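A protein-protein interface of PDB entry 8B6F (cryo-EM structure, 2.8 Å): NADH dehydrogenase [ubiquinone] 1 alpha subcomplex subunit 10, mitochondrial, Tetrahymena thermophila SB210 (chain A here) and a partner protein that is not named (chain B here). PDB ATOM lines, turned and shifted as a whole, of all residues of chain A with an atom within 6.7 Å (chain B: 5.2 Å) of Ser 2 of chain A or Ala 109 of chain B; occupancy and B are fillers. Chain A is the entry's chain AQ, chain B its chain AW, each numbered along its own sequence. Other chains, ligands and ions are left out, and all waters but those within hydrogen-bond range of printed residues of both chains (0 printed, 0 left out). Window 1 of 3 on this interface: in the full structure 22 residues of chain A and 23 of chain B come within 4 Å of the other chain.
OG of Ser 110 of chain A lies within hydrogen-bond range of N of Glu 107 of chain B.
The side-chain carboxylate of Glu 107 of chain B lies within salt-bridge range of the guanidinium group of Arg 45 of chain A (2.6 Å).
N of Gly 23 of chain A sits at hydrogen-bond distance from OD2 of Asp 110 of chain B (3.5 Å).
The guanidinium group of Arg 41 of chain A lies within salt-bridge range of the side-chain carboxylate of Asp 110 of chain B (2.7 Å).
Of chain B, only Ala 109 comes within 4 Å of Ser 2 of chain A.
Of the printed residues of chain B, Arg 41 of chain A touches Asp 110 (2.7 Å) and Leu 113 (3.2 Å).
Of the printed residues of chain A, Asp 110 of chain B touches Gly 23 and Arg 41.
Of the printed residues of chain B, Arg 111 of chain A touches Glu 107.
Printed residues of chain B within 4 Å of Gly 23 of chain A: Asp 110 (3.5 Å).
Of the printed residues of chain A, Leu 113 of chain B touches Arg 41.
Pro 112 of chain A touches none of the printed residues of chain B.
Tyr 6 of chain A touches none of the printed residues of chain B.
The nearest residue of chain B that does not touch Ser 2 of chain A is Asp 110 of chain B (4.7 Å).
The nearest residue of chain A that does not touch Ala 109 of chain B is Arg 41 of chain A (6.1 Å).
Among the printed residues, merely in contact across the chains: Ser 2 of chain A with Ala 109 of chain B (3.3 Å), Arg 41 of chain A with Leu 113 of chain B (3.2 Å) and Arg 111 of chain A with Glu 107 of chain B (3.6 Å).
Along chain B the printed residues that touch a printed residue of chain A span positions 107 to 113.
NH2 of Arg 111 of chain A lies within hydrogen-bond range of OH of Tyr 6 of chain A, 3.0 Å away.
NE of Arg 111 of chain A sits at hydrogen-bond distance from O of Ser 2 of chain A (3.3 Å).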
ATOM      1  N   SER A   2     -26.771   7.987  -8.695  1.00  0.00           N
ATOM      2  CA  SER A   2     -26.991   7.009  -7.593  1.00  0.00           C
ATOM      3  C   SER A   2     -26.356   5.671  -7.943  1.00  0.00           C
ATOM      4  O   SER A   2     -26.369   5.258  -9.099  1.00  0.00           O
ATOM      5  CB  SER A   2     -28.485   6.836  -7.323  1.00  0.00           C
ATOM      6  OG  SER A   2     -29.079   8.066  -6.947  1.00  0.00           O
ATOM      7  N   LYS A   3     -25.809   4.991  -6.935  1.00  0.00           N
ATOM      8  CA  LYS A   3     -25.068   3.759  -7.172  1.00  0.00           C
ATOM      9  C   LYS A   3     -25.967   2.570  -7.486  1.00  0.00           C
ATOM     10  O   LYS A   3     -25.460   1.551  -7.963  1.00  0.00           O
ATOM     11  CB  LYS A   3     -24.187   3.434  -5.965  1.00  0.00           C
ATOM     12  CG  LYS A   3     -22.980   4.350  -5.837  1.00  0.00           C
ATOM     13  CD  LYS A   3     -22.040   3.885  -4.741  1.00  0.00           C
ATOM     14  CE  LYS A   3     -20.814   4.778  -4.659  1.00  0.00           C
ATOM     15  NZ  LYS A   3     -19.876   4.341  -3.588  1.00  0.00           N
ATOM     16  N   ALA A   4     -27.269   2.666  -7.232  1.00  0.00           N
ATOM     17  CA  ALA A   4     -28.211   1.615  -7.613  1.00  0.00           C
ATOM     18  C   ALA A   4     -27.788   0.261  -7.053  1.00  0.00           C
ATOM     19  O   ALA A   4     -27.865  -0.766  -7.729  1.00  0.00           O
ATOM     20  CB  ALA A   4     -28.359   1.541  -9.132  1.00  0.00           C
ATOM     21  N   TYR A   5     -27.338   0.260  -5.801  1.00  0.00           N
ATOM     22  CA  TYR A   5     -26.916  -0.954  -5.116  1.00  0.00           C
ATOM     23  C   TYR A   5     -27.876  -1.327  -3.990  1.00  0.00           C
ATOM     24  O   TYR A   5     -27.461  -1.853  -2.957  1.00  0.00           O
ATOM     25  CB  TYR A   5     -25.485  -0.812  -4.590  1.00  0.00           C
ATOM     26  CG  TYR A   5     -25.214   0.356  -3.648  1.00  0.00           C
ATOM     27  CD1 TYR A   5     -26.240   1.142  -3.134  1.00  0.00           C
ATOM     28  CD2 TYR A   5     -23.913   0.665  -3.277  1.00  0.00           C
ATOM     29  CE1 TYR A   5     -25.976   2.196  -2.283  1.00  0.00           C
ATOM     30  CE2 TYR A   5     -23.640   1.717  -2.427  1.00  0.00           C
ATOM     31  CZ  TYR A   5     -24.675   2.478  -1.934  1.00  0.00           C
ATOM     32  OH  TYR A   5     -24.406   3.526  -1.086  1.00  0.00           O
ATOM     33  N   TYR A   6     -29.171  -1.067  -4.189  1.00  0.00           N
ATOM     34  CA  TYR A   6     -30.149  -1.320  -3.137  1.00  0.00           C
ATOM     35  C   TYR A   6     -30.225  -2.798  -2.788  1.00  0.00           C
ATOM     36  O   TYR A   6     -30.256  -3.166  -1.608  1.00  0.00           O
ATOM     37  CB  TYR A   6     -31.529  -0.815  -3.554  1.00  0.00           C
ATOM     38  CG  TYR A   6     -31.554   0.557  -4.179  1.00  0.00           C
ATOM     39  CD1 TYR A   6     -31.418   1.688  -3.393  1.00  0.00           C
ATOM     40  CD2 TYR A   6     -31.746   0.726  -5.545  1.00  0.00           C
ATOM     41  CE1 TYR A   6     -31.453   2.945  -3.940  1.00  0.00           C
ATOM     42  CE2 TYR A   6     -31.785   1.990  -6.106  1.00  0.00           C
ATOM     43  CZ  TYR A   6     -31.646   3.096  -5.289  1.00  0.00           C
ATOM     44  OH  TYR A   6     -31.676   4.372  -5.799  1.00  0.00           O
ATOM     45  N   LEU A  19     -32.409   4.954   1.120  1.00  0.00           N
ATOM     46  CA  LEU A  19     -31.741   5.135  -0.164  1.00  0.00           C
ATOM     47  C   LEU A  19     -32.733   5.524  -1.253  1.00  0.00           C
ATOM     48  O   LEU A  19     -32.436   6.376  -2.096  1.00  0.00           O
ATOM     49  CB  LEU A  19     -31.001   3.856  -0.554  1.00  0.00           C
ATOM     50  CG  LEU A  19     -29.754   3.502   0.259  1.00  0.00           C
ATOM     51  CD1 LEU A  19     -29.320   2.077  -0.024  1.00  0.00           C
ATOM     52  CD2 LEU A  19     -28.625   4.470  -0.046  1.00  0.00           C
ATOM     53  N   GLY A  23     -31.000  10.189  -1.484  1.00  0.00           N
ATOM     54  CA  GLY A  23     -29.803   9.559  -2.013  1.00  0.00           C
ATOM     55  C   GLY A  23     -28.911   8.952  -0.951  1.00  0.00           C
ATOM     56  O   GLY A  23     -28.076   8.100  -1.269  1.00  0.00           O
ATOM     57  N   ARG A  41     -38.113  14.583  -5.515  1.00  0.00           N
ATOM     58  CA  ARG A  41     -37.562  13.951  -6.707  1.00  0.00           C
ATOM     59  C   ARG A  41     -37.856  12.459  -6.718  1.00  0.00           C
ATOM     60  O   ARG A  41     -38.234  11.898  -7.753  1.00  0.00           O
ATOM     61  CB  ARG A  41     -36.057  14.198  -6.778  1.00  0.00           C
ATOM     62  CG  ARG A  41     -35.433  13.806  -8.102  1.00  0.00           C
ATOM     63  CD  ARG A  41     -33.922  13.753  -8.003  1.00  0.00           C
ATOM     64  NE  ARG A  41     -33.389  14.894  -7.270  1.00  0.00           N
ATOM     65  CZ  ARG A  41     -33.219  16.105  -7.784  1.00  0.00           C
ATOM     66  NH1 ARG A  41     -33.546  16.377  -9.035  1.00  0.00           N
ATOM     67  NH2 ARG A  41     -32.707  17.066  -7.021  1.00  0.00           N
ATOM     68  N   ARG A  45     -40.120  10.515  -9.444  1.00  0.00           N
ATOM     69  CA  ARG A  45     -39.528   9.426 -10.209  1.00  0.00           C
ATOM     70  C   ARG A  45     -40.383   8.169 -10.115  1.00  0.00           C
ATOM     71  O   ARG A  45     -40.632   7.498 -11.124  1.00  0.00           O
ATOM     72  CB  ARG A  45     -38.111   9.153  -9.703  1.00  0.00           C
ATOM     73  CG  ARG A  45     -37.365   8.089 -10.487  1.00  0.00           C
ATOM     74  CD  ARG A  45     -36.021   7.778  -9.852  1.00  0.00           C
ATOM     75  NE  ARG A  45     -35.165   8.955  -9.770  1.00  0.00           N
ATOM     76  CZ  ARG A  45     -34.393   9.392 -10.755  1.00  0.00           C
ATOM     77  NH1 ARG A  45     -34.352   8.779 -11.926  1.00  0.00           N
ATOM     78  NH2 ARG A  45     -33.641  10.471 -10.559  1.00  0.00           N
ATOM     79  N   SER A 110     -27.061   3.698 -17.064  1.00  0.00           N
ATOM     80  CA  SER A 110     -26.066   4.731 -16.814  1.00  0.00           C
ATOM     81  C   SER A 110     -25.648   4.816 -15.354  1.00  0.00           C
ATOM     82  O   SER A 110     -24.801   5.651 -15.018  1.00  0.00           O
ATOM     83  CB  SER A 110     -26.607   6.082 -17.280  1.00  0.00           C
ATOM     84  OG  SER A 110     -27.709   6.481 -16.490  1.00  0.00           O
ATOM     85  N   ARG A 111     -26.217   3.995 -14.488  1.00  0.00           N
ATOM     86  CA  ARG A 111     -25.912   4.044 -13.070  1.00  0.00           C
ATOM     87  C   ARG A 111     -24.983   2.903 -12.672  1.00  0.00           C
ATOM     88  O   ARG A 111     -25.006   1.833 -13.287  1.00  0.00           O
ATOM     89  CB  ARG A 111     -27.204   3.956 -12.259  1.00  0.00           C
ATOM     90  CG  ARG A 111     -28.173   5.088 -12.538  1.00  0.00           C
ATOM     91  CD  ARG A 111     -29.504   4.810 -11.894  1.00  0.00           C
ATOM     92  NE  ARG A 111     -29.363   4.663 -10.455  1.00  0.00           N
ATOM     93  CZ  ARG A 111     -30.360   4.390  -9.627  1.00  0.00           C
ATOM     94  NH1 ARG A 111     -31.598   4.228 -10.063  1.00  0.00           N
ATOM     95  NH2 ARG A 111     -30.100   4.248  -8.333  1.00  0.00           N
ATOM     96  N   PRO A 112     -24.150   3.090 -11.648  1.00  0.00           N
ATOM     97  CA  PRO A 112     -23.305   1.986 -11.182  1.00  0.00           C
ATOM     98  C   PRO A 112     -24.136   0.815 -10.681  1.00  0.00           C
ATOM     99  O   PRO A 112     -25.320   0.943 -10.370  1.00  0.00           O
ATOM    100  CB  PRO A 112     -22.489   2.614 -10.047  1.00  0.00           C
ATOM    101  CG  PRO A 112     -22.497   4.066 -10.330  1.00  0.00           C
ATOM    102  CD  PRO A 112     -23.820   4.354 -10.966  1.00  0.00           C
ATOM    103  N   TYR A 113     -23.496  -0.350 -10.630  1.00  0.00           N
ATOM    104  CA  TYR A 113     -24.089  -1.591 -10.140  1.00  0.00           C
ATOM    105  C   TYR A 113     -25.315  -2.019 -10.935  1.00  0.00           C
ATOM    106  O   TYR A 113     -26.027  -2.938 -10.516  1.00  0.00           O
ATOM    107  CB  TYR A 113     -24.455  -1.487  -8.656  1.00  0.00           C
ATOM    108  CG  TYR A 113     -23.263  -1.389  -7.735  1.00  0.00           C
ATOM    109  CD1 TYR A 113     -22.660  -2.531  -7.227  1.00  0.00           C
ATOM    110  CD2 TYR A 113     -22.748  -0.156  -7.362  1.00  0.00           C
ATOM    111  CE1 TYR A 113     -21.575  -2.449  -6.381  1.00  0.00           C
ATOM    112  CE2 TYR A 113     -21.663  -0.063  -6.517  1.00  0.00           C
ATOM    113  CZ  TYR A 113     -21.081  -1.213  -6.030  1.00  0.00           C
ATOM    114  OH  TYR A 113     -19.999  -1.126  -5.187  1.00  0.00           O
ATOM    115  N   GLU B 107     -29.065   9.180 -15.975  1.00  0.00           N
ATOM    116  CA  GLU B 107     -29.523   9.376 -14.607  1.00  0.00           C
ATOM    117  C   GLU B 107     -28.502  10.223 -13.865  1.00  0.00           C
ATOM    118  O   GLU B 107     -27.307   9.911 -13.878  1.00  0.00           O
ATOM    119  CB  GLU B 107     -29.716   8.037 -13.890  1.00  0.00           C
ATOM    120  CG  GLU B 107     -30.797   7.160 -14.495  1.00  0.00           C
ATOM    121  CD  GLU B 107     -32.177   7.766 -14.372  1.00  0.00           C
ATOM    122  OE1 GLU B 107     -32.339   8.715 -13.579  1.00  0.00           O
ATOM    123  OE2 GLU B 107     -33.100   7.292 -15.066  1.00  0.00           O
ATOM    124  N   LEU B 108     -28.971  11.285 -13.220  1.00  0.00           N
ATOM    125  CA  LEU B 108     -28.115  12.210 -12.492  1.00  0.00           C
ATOM    126  C   LEU B 108     -28.305  11.998 -10.998  1.00  0.00           C
ATOM    127  O   LEU B 108     -29.439  11.975 -10.508  1.00  0.00           O
ATOM    128  CB  LEU B 108     -28.431  13.657 -12.873  1.00  0.00           C
ATOM    129  CG  LEU B 108     -28.248  14.001 -14.353  1.00  0.00           C
ATOM    130  CD1 LEU B 108     -28.727  15.414 -14.640  1.00  0.00           C
ATOM    131  CD2 LEU B 108     -26.797  13.836 -14.774  1.00  0.00           C
ATOM    132  N   ALA B 109     -27.197  11.842 -10.280  1.00  0.00           N
ATOM    133  CA  ALA B 109     -27.259  11.617  -8.845  1.00  0.00           C
ATOM    134  C   ALA B 109     -27.669  12.892  -8.118  1.00  0.00           C
ATOM    135  O   ALA B 109     -27.430  14.008  -8.584  1.00  0.00           O
ATOM    136  CB  ALA B 109     -25.907  11.135  -8.322  1.00  0.00           C
ATOM    137  N   ASP B 110     -28.296  12.714  -6.952  1.00  0.00           N
ATOM    138  CA  ASP B 110     -28.691  13.865  -6.148  1.00  0.00           C
ATOM    139  C   ASP B 110     -27.485  14.716  -5.781  1.00  0.00           C
ATOM    140  O   ASP B 110     -27.574  15.947  -5.740  1.00  0.00           O
ATOM    141  CB  ASP B 110     -29.421  13.403  -4.887  1.00  0.00           C
ATOM    142  CG  ASP B 110     -30.824  12.903  -5.173  1.00  0.00           C
ATOM    143  OD1 ASP B 110     -31.477  13.449  -6.087  1.00  0.00           O
ATOM    144  OD2 ASP B 110     -31.276  11.966  -4.484  1.00  0.00           O
ATOM    145  N   GLU B 111     -26.345  14.077  -5.512  1.00  0.00           N
ATOM    146  CA  GLU B 111     -25.144  14.831  -5.172  1.00  0.00           C
ATOM    147  C   GLU B 111     -24.735  15.746  -6.318  1.00  0.00           C
ATOM    148  O   GLU B 111     -24.421  16.923  -6.108  1.00  0.00           O
ATOM    149  CB  GLU B 111     -24.005  13.876  -4.813  1.00  0.00           C
ATOM    150  CG  GLU B 111     -24.183  13.153  -3.484  1.00  0.00           C
ATOM    151  CD  GLU B 111     -25.213  12.039  -3.549  1.00  0.00           C
ATOM    152  OE1 GLU B 111     -25.811  11.840  -4.627  1.00  0.00           O
ATOM    153  OE2 GLU B 111     -25.422  11.361  -2.521  1.00  0.00           O
ATOM    154  N   ASP B 112     -24.725  15.220  -7.545  1.00  0.00           N
ATOM    155  CA  ASP B 112     -24.352  16.042  -8.692  1.00  0.00           C
ATOM    156  C   ASP B 112     -25.370  17.145  -8.939  1.00  0.00           C
ATOM    157  O   ASP B 112     -24.996  18.287  -9.231  1.00  0.00           O
ATOM    158  CB  ASP B 112     -24.209  15.166  -9.936  1.00  0.00           C
ATOM    159  CG  ASP B 112     -23.221  14.035  -9.741  1.00  0.00           C
ATOM    160  OD1 ASP B 112     -22.278  14.199  -8.940  1.00  0.00           O
ATOM    161  OD2 ASP B 112     -23.388  12.979 -10.388  1.00  0.00           O
ATOM    162  N   LEU B 113     -26.659  16.829  -8.822  1.00  0.00           N
ATOM    163  CA  LEU B 113     -27.691  17.836  -9.049  1.00  0.00           C
ATOM    164  C   LEU B 113     -27.593  18.961  -8.028  1.00  0.00           C
ATOM    165  O   LEU B 113     -27.799  20.133  -8.361  1.00  0.00           O
ATOM    166  CB  LEU B 113     -29.072  17.185  -9.013  1.00  0.00           C
ATOM    167  CG  LEU B 113     -29.316  16.144 -10.109  1.00  0.00           C
ATOM    168  CD1 LEU B 113     -30.626  15.434  -9.889  1.00  0.00           C
ATOM    169  CD2 LEU B 113     -29.302  16.792 -11.480  1.00  0.00           C
ATOM    170  N   GLU B 114     -27.284  18.622  -6.776  1.00  0.00           N
ATOM    171  CA  GLU B 114     -27.115  19.646  -5.753  1.00  0.00           C
ATOM    172  C   GLU B 114     -25.821  20.422  -5.943  1.00  0.00           C
ATOM    173  O   GLU B 114     -25.754  21.607  -5.601  1.00  0.00           O
ATOM    174  CB  GLU B 114     -27.159  19.009  -4.364  1.00  0.00           C
ATOM    175  CG  GLU B 114     -28.506  18.388  -4.025  1.00  0.00           C
ATOM    176  CD  GLU B 114     -28.486  17.615  -2.723  1.00  0.00           C
ATOM    177  OE1 GLU B 114     -27.435  17.605  -2.050  1.00  0.00           O
ATOM    178  OE2 GLU B 114     -29.524  17.018  -2.371  1.00  0.00           O
